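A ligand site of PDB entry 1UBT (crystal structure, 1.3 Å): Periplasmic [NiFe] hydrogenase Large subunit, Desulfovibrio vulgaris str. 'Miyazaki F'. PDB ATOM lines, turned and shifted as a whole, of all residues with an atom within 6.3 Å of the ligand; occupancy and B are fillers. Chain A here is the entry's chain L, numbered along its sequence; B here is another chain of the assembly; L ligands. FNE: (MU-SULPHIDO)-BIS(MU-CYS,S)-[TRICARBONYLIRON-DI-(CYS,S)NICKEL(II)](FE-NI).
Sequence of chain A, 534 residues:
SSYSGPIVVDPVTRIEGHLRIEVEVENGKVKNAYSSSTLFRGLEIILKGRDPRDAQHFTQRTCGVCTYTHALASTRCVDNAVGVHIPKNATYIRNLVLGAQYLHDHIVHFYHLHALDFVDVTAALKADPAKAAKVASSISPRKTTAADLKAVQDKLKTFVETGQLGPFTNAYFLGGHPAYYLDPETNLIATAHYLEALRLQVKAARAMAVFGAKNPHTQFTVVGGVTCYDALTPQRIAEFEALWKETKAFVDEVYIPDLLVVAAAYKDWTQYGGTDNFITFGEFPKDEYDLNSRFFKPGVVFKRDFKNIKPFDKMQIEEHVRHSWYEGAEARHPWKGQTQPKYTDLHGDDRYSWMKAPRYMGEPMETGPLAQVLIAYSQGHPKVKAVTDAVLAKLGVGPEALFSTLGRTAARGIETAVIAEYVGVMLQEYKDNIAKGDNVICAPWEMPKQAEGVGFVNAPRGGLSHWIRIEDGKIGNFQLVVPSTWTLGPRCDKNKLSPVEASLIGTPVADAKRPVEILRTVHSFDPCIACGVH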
ATOM      1  N   GLU A  16       7.002   2.148  22.248  1.00  0.00           N
ATOM      2  CA  GLU A  16       6.477   3.458  22.538  1.00  0.00           C
ATOM      3  C   GLU A  16       5.597   3.343  23.795  1.00  0.00           C
ATOM      4  O   GLU A  16       4.681   2.562  23.882  1.00  0.00           O
ATOM      5  CB  GLU A  16       5.682   4.026  21.383  1.00  0.00           C
ATOM      6  CG  GLU A  16       5.294   5.506  21.438  1.00  0.00           C
ATOM      7  CD  GLU A  16       4.326   5.937  22.516  1.00  0.00           C
ATOM      8  OE1 GLU A  16       4.494   6.933  23.247  1.00  0.00           O
ATOM      9  OE2 GLU A  16       3.482   5.047  22.764  1.00  0.00           O
ATOM     10  N   THR A  62      -1.601  11.730  19.422  1.00  0.00           N
ATOM     11  CA  THR A  62      -1.737  10.419  20.055  1.00  0.00           C
ATOM     12  C   THR A  62      -0.376   9.715  20.118  1.00  0.00           C
ATOM     13  O   THR A  62       0.007   9.066  21.082  1.00  0.00           O
ATOM     14  CB  THR A  62      -2.714   9.505  19.298  1.00  0.00           C
ATOM     15  OG1 THR A  62      -4.018  10.098  19.413  1.00  0.00           O
ATOM     16  CG2 THR A  62      -2.721   8.122  19.908  1.00  0.00           C
ATOM     17  N   CYS A  63       0.372   9.853  19.021  1.00  0.00           N
ATOM     18  CA  CYS A  63       1.616   9.125  18.876  1.00  0.00           C
ATOM     19  C   CYS A  63       2.514   9.740  17.774  1.00  0.00           C
ATOM     20  O   CYS A  63       2.071  10.019  16.659  1.00  0.00           O
ATOM     21  CB  CYS A  63       1.282   7.694  18.547  1.00  0.00           C
ATOM     22  SG  CYS A  63       2.794   6.641  18.477  1.00  0.00           S
ATOM     23  N   GLY A  64       3.794   9.933  18.141  1.00  0.00           N
ATOM     24  CA  GLY A  64       4.831  10.430  17.245  1.00  0.00           C
ATOM     25  C   GLY A  64       5.722   9.372  16.634  1.00  0.00           C
ATOM     26  O   GLY A  64       6.565   9.705  15.828  1.00  0.00           O
ATOM     27  N   VAL A  65       5.513   8.124  17.034  1.00  0.00           N
ATOM     28  CA  VAL A  65       6.176   6.973  16.403  1.00  0.00           C
ATOM     29  C   VAL A  65       5.364   6.673  15.143  1.00  0.00           C
ATOM     30  O   VAL A  65       5.838   6.789  14.005  1.00  0.00           O
ATOM     31  CB  VAL A  65       6.328   5.787  17.339  1.00  0.00           C
ATOM     32  CG1 VAL A  65       6.904   4.567  16.620  1.00  0.00           C
ATOM     33  CG2 VAL A  65       7.202   6.179  18.528  1.00  0.00           C
ATOM     34  N   CYS A  66       4.086   6.307  15.351  1.00  0.00           N
ATOM     35  CA  CYS A  66       3.137   6.229  14.235  1.00  0.00           C
ATOM     36  C   CYS A  66       2.569   7.620  13.955  1.00  0.00           C
ATOM     37  O   CYS A  66       1.409   7.854  13.868  1.00  0.00           O
ATOM     38  CB  CYS A  66       2.068   5.200  14.463  1.00  0.00           C
ATOM     39  SG  CYS A  66       0.934   5.464  15.836  1.00  0.00           S
ATOM     40  N   THR A  67       3.494   8.568  13.783  1.00  0.00           N
ATOM     41  CA  THR A  67       3.109   9.907  13.371  1.00  0.00           C
ATOM     42  C   THR A  67       2.364   9.817  12.035  1.00  0.00           C
ATOM     43  O   THR A  67       2.433   8.795  11.357  1.00  0.00           O
ATOM     44  CB  THR A  67       4.347  10.800  13.328  1.00  0.00           C
ATOM     45  OG1 THR A  67       3.888  12.136  13.125  1.00  0.00           O
ATOM     46  CG2 THR A  67       5.289  10.473  12.156  1.00  0.00           C
ATOM     47  N   THR A  69      -0.350   8.823  11.026  1.00  0.00           N
ATOM     48  CA  THR A  69      -1.461   7.892  10.940  1.00  0.00           C
ATOM     49  C   THR A  69      -2.754   8.388  11.580  1.00  0.00           C
ATOM     50  O   THR A  69      -3.838   8.181  11.016  1.00  0.00           O
ATOM     51  CB  THR A  69      -1.119   6.512  11.550  1.00  0.00           C
ATOM     52  OG1 THR A  69      -0.935   6.640  12.958  1.00  0.00           O
ATOM     53  CG2 THR A  69       0.126   5.924  10.894  1.00  0.00           C
ATOM     54  N   HIS A  70      -2.662   9.045  12.718  1.00  0.00           N
ATOM     55  CA  HIS A  70      -3.886   9.561  13.334  1.00  0.00           C
ATOM     56  C   HIS A  70      -4.391  10.806  12.639  1.00  0.00           C
ATOM     57  O   HIS A  70      -5.616  11.009  12.643  1.00  0.00           O
ATOM     58  CB  HIS A  70      -3.671   9.806  14.842  1.00  0.00           C
ATOM     59  CG  HIS A  70      -3.449   8.560  15.630  1.00  0.00           C
ATOM     60  ND1 HIS A  70      -4.531   7.802  16.075  1.00  0.00           N
ATOM     61  CD2 HIS A  70      -2.319   7.924  16.028  1.00  0.00           C
ATOM     62  CE1 HIS A  70      -4.052   6.760  16.732  1.00  0.00           C
ATOM     63  NE2 HIS A  70      -2.685   6.826  16.722  1.00  0.00           N
ATOM     64  N   ASP A 105       8.909   3.214   9.958  1.00  0.00           N
ATOM     65  CA  ASP A 105       8.463   2.631  11.211  1.00  0.00           C
ATOM     66  C   ASP A 105       8.981   1.206  11.372  1.00  0.00           C
ATOM     67  O   ASP A 105       9.624   0.862  12.377  1.00  0.00           O
ATOM     68  CB  ASP A 105       6.933   2.736  11.275  1.00  0.00           C
ATOM     69  CG  ASP A 105       6.306   2.644  12.640  1.00  0.00           C
ATOM     70  OD1 ASP A 105       6.951   2.049  13.563  1.00  0.00           O
ATOM     71  OD2 ASP A 105       5.189   3.186  12.795  1.00  0.00           O
ATOM     72  N   ALA A 459      -2.596   0.975  10.019  1.00  0.00           N
ATOM     73  CA  ALA A 459      -1.345   1.607  10.412  1.00  0.00           C
ATOM     74  C   ALA A 459      -0.266   0.540  10.546  1.00  0.00           C
ATOM     75  O   ALA A 459      -0.567  -0.653  10.421  1.00  0.00           O
ATOM     76  CB  ALA A 459      -1.577   2.375  11.730  1.00  0.00           C
ATOM     77  N   PRO A 460       0.991   0.905  10.729  1.00  0.00           N
ATOM     78  CA  PRO A 460       2.051  -0.121  10.909  1.00  0.00           C
ATOM     79  C   PRO A 460       1.722  -1.144  11.997  1.00  0.00           C
ATOM     80  O   PRO A 460       2.273  -2.270  11.906  1.00  0.00           O
ATOM     81  CB  PRO A 460       3.308   0.723  11.217  1.00  0.00           C
ATOM     82  CG  PRO A 460       3.012   1.976  10.407  1.00  0.00           C
ATOM     83  CD  PRO A 460       1.542   2.254  10.689  1.00  0.00           C
ATOM     84  N   ARG A 461       0.927  -0.824  13.011  1.00  0.00           N
ATOM     85  CA  ARG A 461       0.560  -1.792  14.066  1.00  0.00           C
ATOM     86  C   ARG A 461      -0.852  -2.381  13.869  1.00  0.00           C
ATOM     87  O   ARG A 461      -1.247  -3.221  14.676  1.00  0.00           O
ATOM     88  CB  ARG A 461       0.724  -1.147  15.465  1.00  0.00           C
ATOM     89  CG  ARG A 461       2.202  -0.850  15.737  1.00  0.00           C
ATOM     90  CD  ARG A 461       2.399   0.201  16.852  1.00  0.00           C
ATOM     91  NE  ARG A 461       3.834   0.453  16.863  1.00  0.00           N
ATOM     92  CZ  ARG A 461       4.468   1.258  16.017  1.00  0.00           C
ATOM     93  NH1 ARG A 461       3.834   1.967  15.082  1.00  0.00           N
ATOM     94  NH2 ARG A 461       5.772   1.368  16.085  1.00  0.00           N
ATOM     95  N   GLY A 462      -1.575  -1.935  12.813  1.00  0.00           N
ATOM     96  CA  GLY A 462      -2.827  -2.589  12.474  1.00  0.00           C
ATOM     97  C   GLY A 462      -4.024  -1.668  12.353  1.00  0.00           C
ATOM     98  O   GLY A 462      -3.892  -0.491  11.986  1.00  0.00           O
ATOM     99  N   GLY A 463      -5.230  -2.208  12.617  1.00  0.00           N
ATOM    100  CA  GLY A 463      -6.417  -1.494  12.269  1.00  0.00           C
ATOM    101  C   GLY A 463      -6.733  -0.331  13.216  1.00  0.00           C
ATOM    102  O   GLY A 463      -7.097  -0.582  14.365  1.00  0.00           O
ATOM    103  N   LEU A 464      -6.648   0.875  12.670  1.00  0.00           N
ATOM    104  CA  LEU A 464      -6.936   2.118  13.357  1.00  0.00           C
ATOM    105  C   LEU A 464      -8.285   2.698  12.925  1.00  0.00           C
ATOM    106  O   LEU A 464      -8.511   2.774  11.719  1.00  0.00           O
ATOM    107  CB  LEU A 464      -5.830   3.108  13.125  1.00  0.00           C
ATOM    108  CG  LEU A 464      -6.056   4.561  13.563  1.00  0.00           C
ATOM    109  CD1 LEU A 464      -6.220   4.632  15.087  1.00  0.00           C
ATOM    110  CD2 LEU A 464      -4.929   5.478  13.067  1.00  0.00           C
ATOM    111  N   VAL A 482      -7.557   1.989  18.656  1.00  0.00           N
ATOM    112  CA  VAL A 482      -6.243   2.028  18.015  1.00  0.00           C
ATOM    113  C   VAL A 482      -5.655   0.636  17.948  1.00  0.00           C
ATOM    114  O   VAL A 482      -6.035  -0.225  18.792  1.00  0.00           O
ATOM    115  CB  VAL A 482      -5.412   3.029  18.830  1.00  0.00           C
ATOM    116  CG1 VAL A 482      -4.054   3.288  18.214  1.00  0.00           C
ATOM    117  CG2 VAL A 482      -6.144   4.375  18.905  1.00  0.00           C
ATOM    118  N   PRO A 483      -4.796   0.280  17.005  1.00  0.00           N
ATOM    119  CA  PRO A 483      -4.309  -1.114  16.927  1.00  0.00           C
ATOM    120  C   PRO A 483      -3.742  -1.650  18.243  1.00  0.00           C
ATOM    121  O   PRO A 483      -4.122  -2.791  18.586  1.00  0.00           O
ATOM    122  CB  PRO A 483      -3.254  -1.087  15.831  1.00  0.00           C
ATOM    123  CG  PRO A 483      -3.247   0.258  15.256  1.00  0.00           C
ATOM    124  CD  PRO A 483      -4.344   1.027  15.862  1.00  0.00           C
ATOM    125  N   SER A 484      -2.893  -0.914  18.941  1.00  0.00           N
ATOM    126  CA  SER A 484      -2.378  -1.459  20.206  1.00  0.00           C
ATOM    127  C   SER A 484      -3.483  -1.611  21.233  1.00  0.00           C
ATOM    128  O   SER A 484      -3.256  -2.384  22.183  1.00  0.00           O
ATOM    129  CB  SER A 484      -1.241  -0.586  20.723  1.00  0.00           C
ATOM    130  OG  SER A 484      -0.106  -0.625  19.911  1.00  0.00           O
ATOM    131  N   THR A 485      -4.598  -0.891  21.122  1.00  0.00           N
ATOM    132  CA  THR A 485      -5.691  -1.149  22.035  1.00  0.00           C
ATOM    133  C   THR A 485      -6.215  -2.579  21.848  1.00  0.00           C
ATOM    134  O   THR A 485      -6.419  -3.313  22.820  1.00  0.00           O
ATOM    135  CB  THR A 485      -6.849  -0.148  21.790  1.00  0.00           C
ATOM    136  OG1 THR A 485      -6.361   1.181  21.515  1.00  0.00           O
ATOM    137  CG2 THR A 485      -7.742  -0.098  23.015  1.00  0.00           C
ATOM    138  N   ASP A 526       5.059  -4.978  18.563  1.00  0.00           N
ATOM    139  CA  ASP A 526       5.386  -3.561  18.319  1.00  0.00           C
ATOM    140  C   ASP A 526       4.416  -2.677  19.103  1.00  0.00           C
ATOM    141  O   ASP A 526       3.676  -1.865  18.558  1.00  0.00           O
ATOM    142  CB  ASP A 526       5.355  -3.289  16.854  1.00  0.00           C
ATOM    143  CG  ASP A 526       5.827  -1.949  16.378  1.00  0.00           C
ATOM    144  OD1 ASP A 526       5.655  -1.714  15.141  1.00  0.00           O
ATOM    145  OD2 ASP A 526       6.361  -1.182  17.209  1.00  0.00           O
ATOM    146  N   PRO A 527       4.384  -2.803  20.435  1.00  0.00           N
ATOM    147  CA  PRO A 527       3.438  -2.024  21.255  1.00  0.00           C
ATOM    148  C   PRO A 527       3.639  -0.519  21.225  1.00  0.00           C
ATOM    149  O   PRO A 527       4.742   0.015  21.202  1.00  0.00           O
ATOM    150  CB  PRO A 527       3.737  -2.489  22.666  1.00  0.00           C
ATOM    151  CG  PRO A 527       4.386  -3.809  22.538  1.00  0.00           C
ATOM    152  CD  PRO A 527       5.221  -3.691  21.256  1.00  0.00           C
ATOM    153  N   CYS A 528       2.490   0.168  21.259  1.00  0.00           N
ATOM    154  CA  CYS A 528       2.471   1.642  21.264  1.00  0.00           C
ATOM    155  C   CYS A 528       1.436   2.050  22.302  1.00  0.00           C
ATOM    156  O   CYS A 528       0.246   1.949  22.027  1.00  0.00           O
ATOM    157  CB  CYS A 528       2.193   2.105  19.829  1.00  0.00           C
ATOM    158  SG  CYS A 528       2.463   3.890  19.741  1.00  0.00           S
ATOM    159  N   ILE A 529       1.874   2.401  23.497  1.00  0.00           N
ATOM    160  CA  ILE A 529       0.925   2.596  24.597  1.00  0.00           C
ATOM    161  C   ILE A 529       0.273   3.973  24.565  1.00  0.00           C
ATOM    162  O   ILE A 529      -0.864   4.099  25.033  1.00  0.00           O
ATOM    163  CB  ILE A 529       1.613   2.313  25.941  1.00  0.00           C
ATOM    164  CG1 ILE A 529       2.466   1.027  25.931  1.00  0.00           C
ATOM    165  CG2 ILE A 529       0.571   2.263  27.060  1.00  0.00           C
ATOM    166  CD1 ILE A 529       1.759  -0.243  25.477  1.00  0.00           C
ATOM    167  N   ALA A 530       0.940   4.972  24.030  1.00  0.00           N
ATOM    168  CA  ALA A 530       0.326   6.271  23.805  1.00  0.00           C
ATOM    169  C   ALA A 530      -0.815   6.102  22.810  1.00  0.00           C
ATOM    170  O   ALA A 530      -1.928   6.600  22.978  1.00  0.00           O
ATOM    171  CB  ALA A 530       1.383   7.240  23.308  1.00  0.00           C
ATOM    172  N   CYS A 531      -0.588   5.323  21.760  1.00  0.00           N
ATOM    173  CA  CYS A 531      -1.628   4.904  20.844  1.00  0.00           C
ATOM    174  C   CYS A 531      -2.745   4.151  21.565  1.00  0.00           C
ATOM    175  O   CYS A 531      -3.919   4.446  21.420  1.00  0.00           O
ATOM    176  CB  CYS A 531      -1.068   3.971  19.757  1.00  0.00           C
ATOM    177  SG  CYS A 531      -0.596   4.942  18.281  1.00  0.00           S
ATOM    178  N   GLY A 532      -2.384   3.117  22.334  1.00  0.00           N
ATOM    179  CA  GLY A 532      -3.456   2.254  22.831  1.00  0.00           C
ATOM    180  C   GLY A 532      -4.384   2.942  23.785  1.00  0.00           C
ATOM    181  O   GLY A 532      -5.567   2.630  23.802  1.00  0.00           O
ATOM    182  N   CYS B  17       3.951  11.605  23.543  1.00  0.00           N
ATOM    183  CA  CYS B  17       3.571  10.807  22.405  1.00  0.00           C
ATOM    184  C   CYS B  17       4.785  10.188  21.699  1.00  0.00           C
ATOM    185  O   CYS B  17       4.624   9.452  20.732  1.00  0.00           O
ATOM    186  CB  CYS B  17       2.805  11.644  21.377  1.00  0.00           C
ATOM    187  SG  CYS B  17       3.840  12.705  20.306  1.00  0.00           S
HETATM  188 NI   FNE L   1       1.786   4.725  17.804  1.00  0.00          NI
HETATM  189 FE   FNE L   1      -0.125   3.576  16.452  1.00  0.00          FE
HETATM  190  C1  FNE L   1      -0.620   1.974  17.447  1.00  0.00           C
HETATM  191  C2  FNE L   1       0.557   2.579  14.923  1.00  0.00           C
HETATM  192  C3  FNE L   1      -1.607   3.765  15.555  1.00  0.00           C
HETATM  193  O1  FNE L   1      -0.847   1.039  18.036  1.00  0.00           O
HETATM  194  O2  FNE L   1       0.914   1.956  14.102  1.00  0.00           O
HETATM  195  O3  FNE L   1      -2.585   3.779  14.996  1.00  0.00           O
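The side-chain sulfur of Cys 528 binds a nickel atom (NI) of the ligand (2.2 Å).
An iron atom (FE) of the ligand is bound by the side-chain sulfur (SG) of Cys 66 (2.3 Å).
SG of Cys 63 binds NI of the ligand (2.3 Å).
An iron atom (FE) of the ligand is bound by the side-chain sulfur of Cys 531 (2.3 Å).
An oxygen (O1) of the ligand sits at hydrogen-bond distance from the backbone NH of Ser 484 (3.0 Å).
The side-chain hydroxyl (OG) of Ser 484 lies within hydrogen-bond range of an oxygen (O1) of the ligand, at 2.6 Å.
The backbone NH of Arg 461 is in hydrogen-bond range of an oxygen (O2) of the ligand, at 3.0 Å.
The guanidinium group of Arg 461 lies within hydrogen-bond range of an oxygen (O2) of the ligand (3.1 Å).
The backbone NH of Cys 528 sits at hydrogen-bond distance from the side-chain hydroxyl of Ser 484 (3.0 Å).
The side-chain sulfur (SG) of Cys 528 sits close to the side-chain carboxylate (OE2) of Glu 16 (3.4 Å).
The side-chain hydroxyl (OG1) of Thr 69 is in hydrogen-bond range of the backbone carbonyl oxygen (O) of Cys 66, 2.8 Å away.
SG of Cys 63 sits close to N of Val 65 (3.4 Å).
The side-chain sulfur (SG) of Cys 531 sits close to a ring nitrogen (NE2) of His 70 (3.2 Å).
The guanidinium group of Arg 461 is in salt-bridge range of the side-chain carboxylate of Asp 105 (2.9 Å).
The side-chain carboxylate (OD2) of Asp 526 lies within salt-bridge range of the guanidinium group (NH2) of Arg 461 (2.8 Å).
O of Val 482 is in hydrogen-bond range of OG1 of Thr 485 (3.1 Å).
Merely in contact with the ligand: Thr 69, His 70, Ala 459, Pro 460, Leu 464, Val 482 and Pro 483.
Hydrophobic or aromatic side chains within 4 Å of the ligand: His 70, Ala 459, Pro 460, Leu 464, Val 482 and Pro 483.
Within 4 Å of the ligand: Cys 63, Cys 66, Thr 69, His 70, Ala 459, Pro 460, Arg 461, Leu 464, Val 482, Pro 483, Ser 484, Cys 528 and Cys 531.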
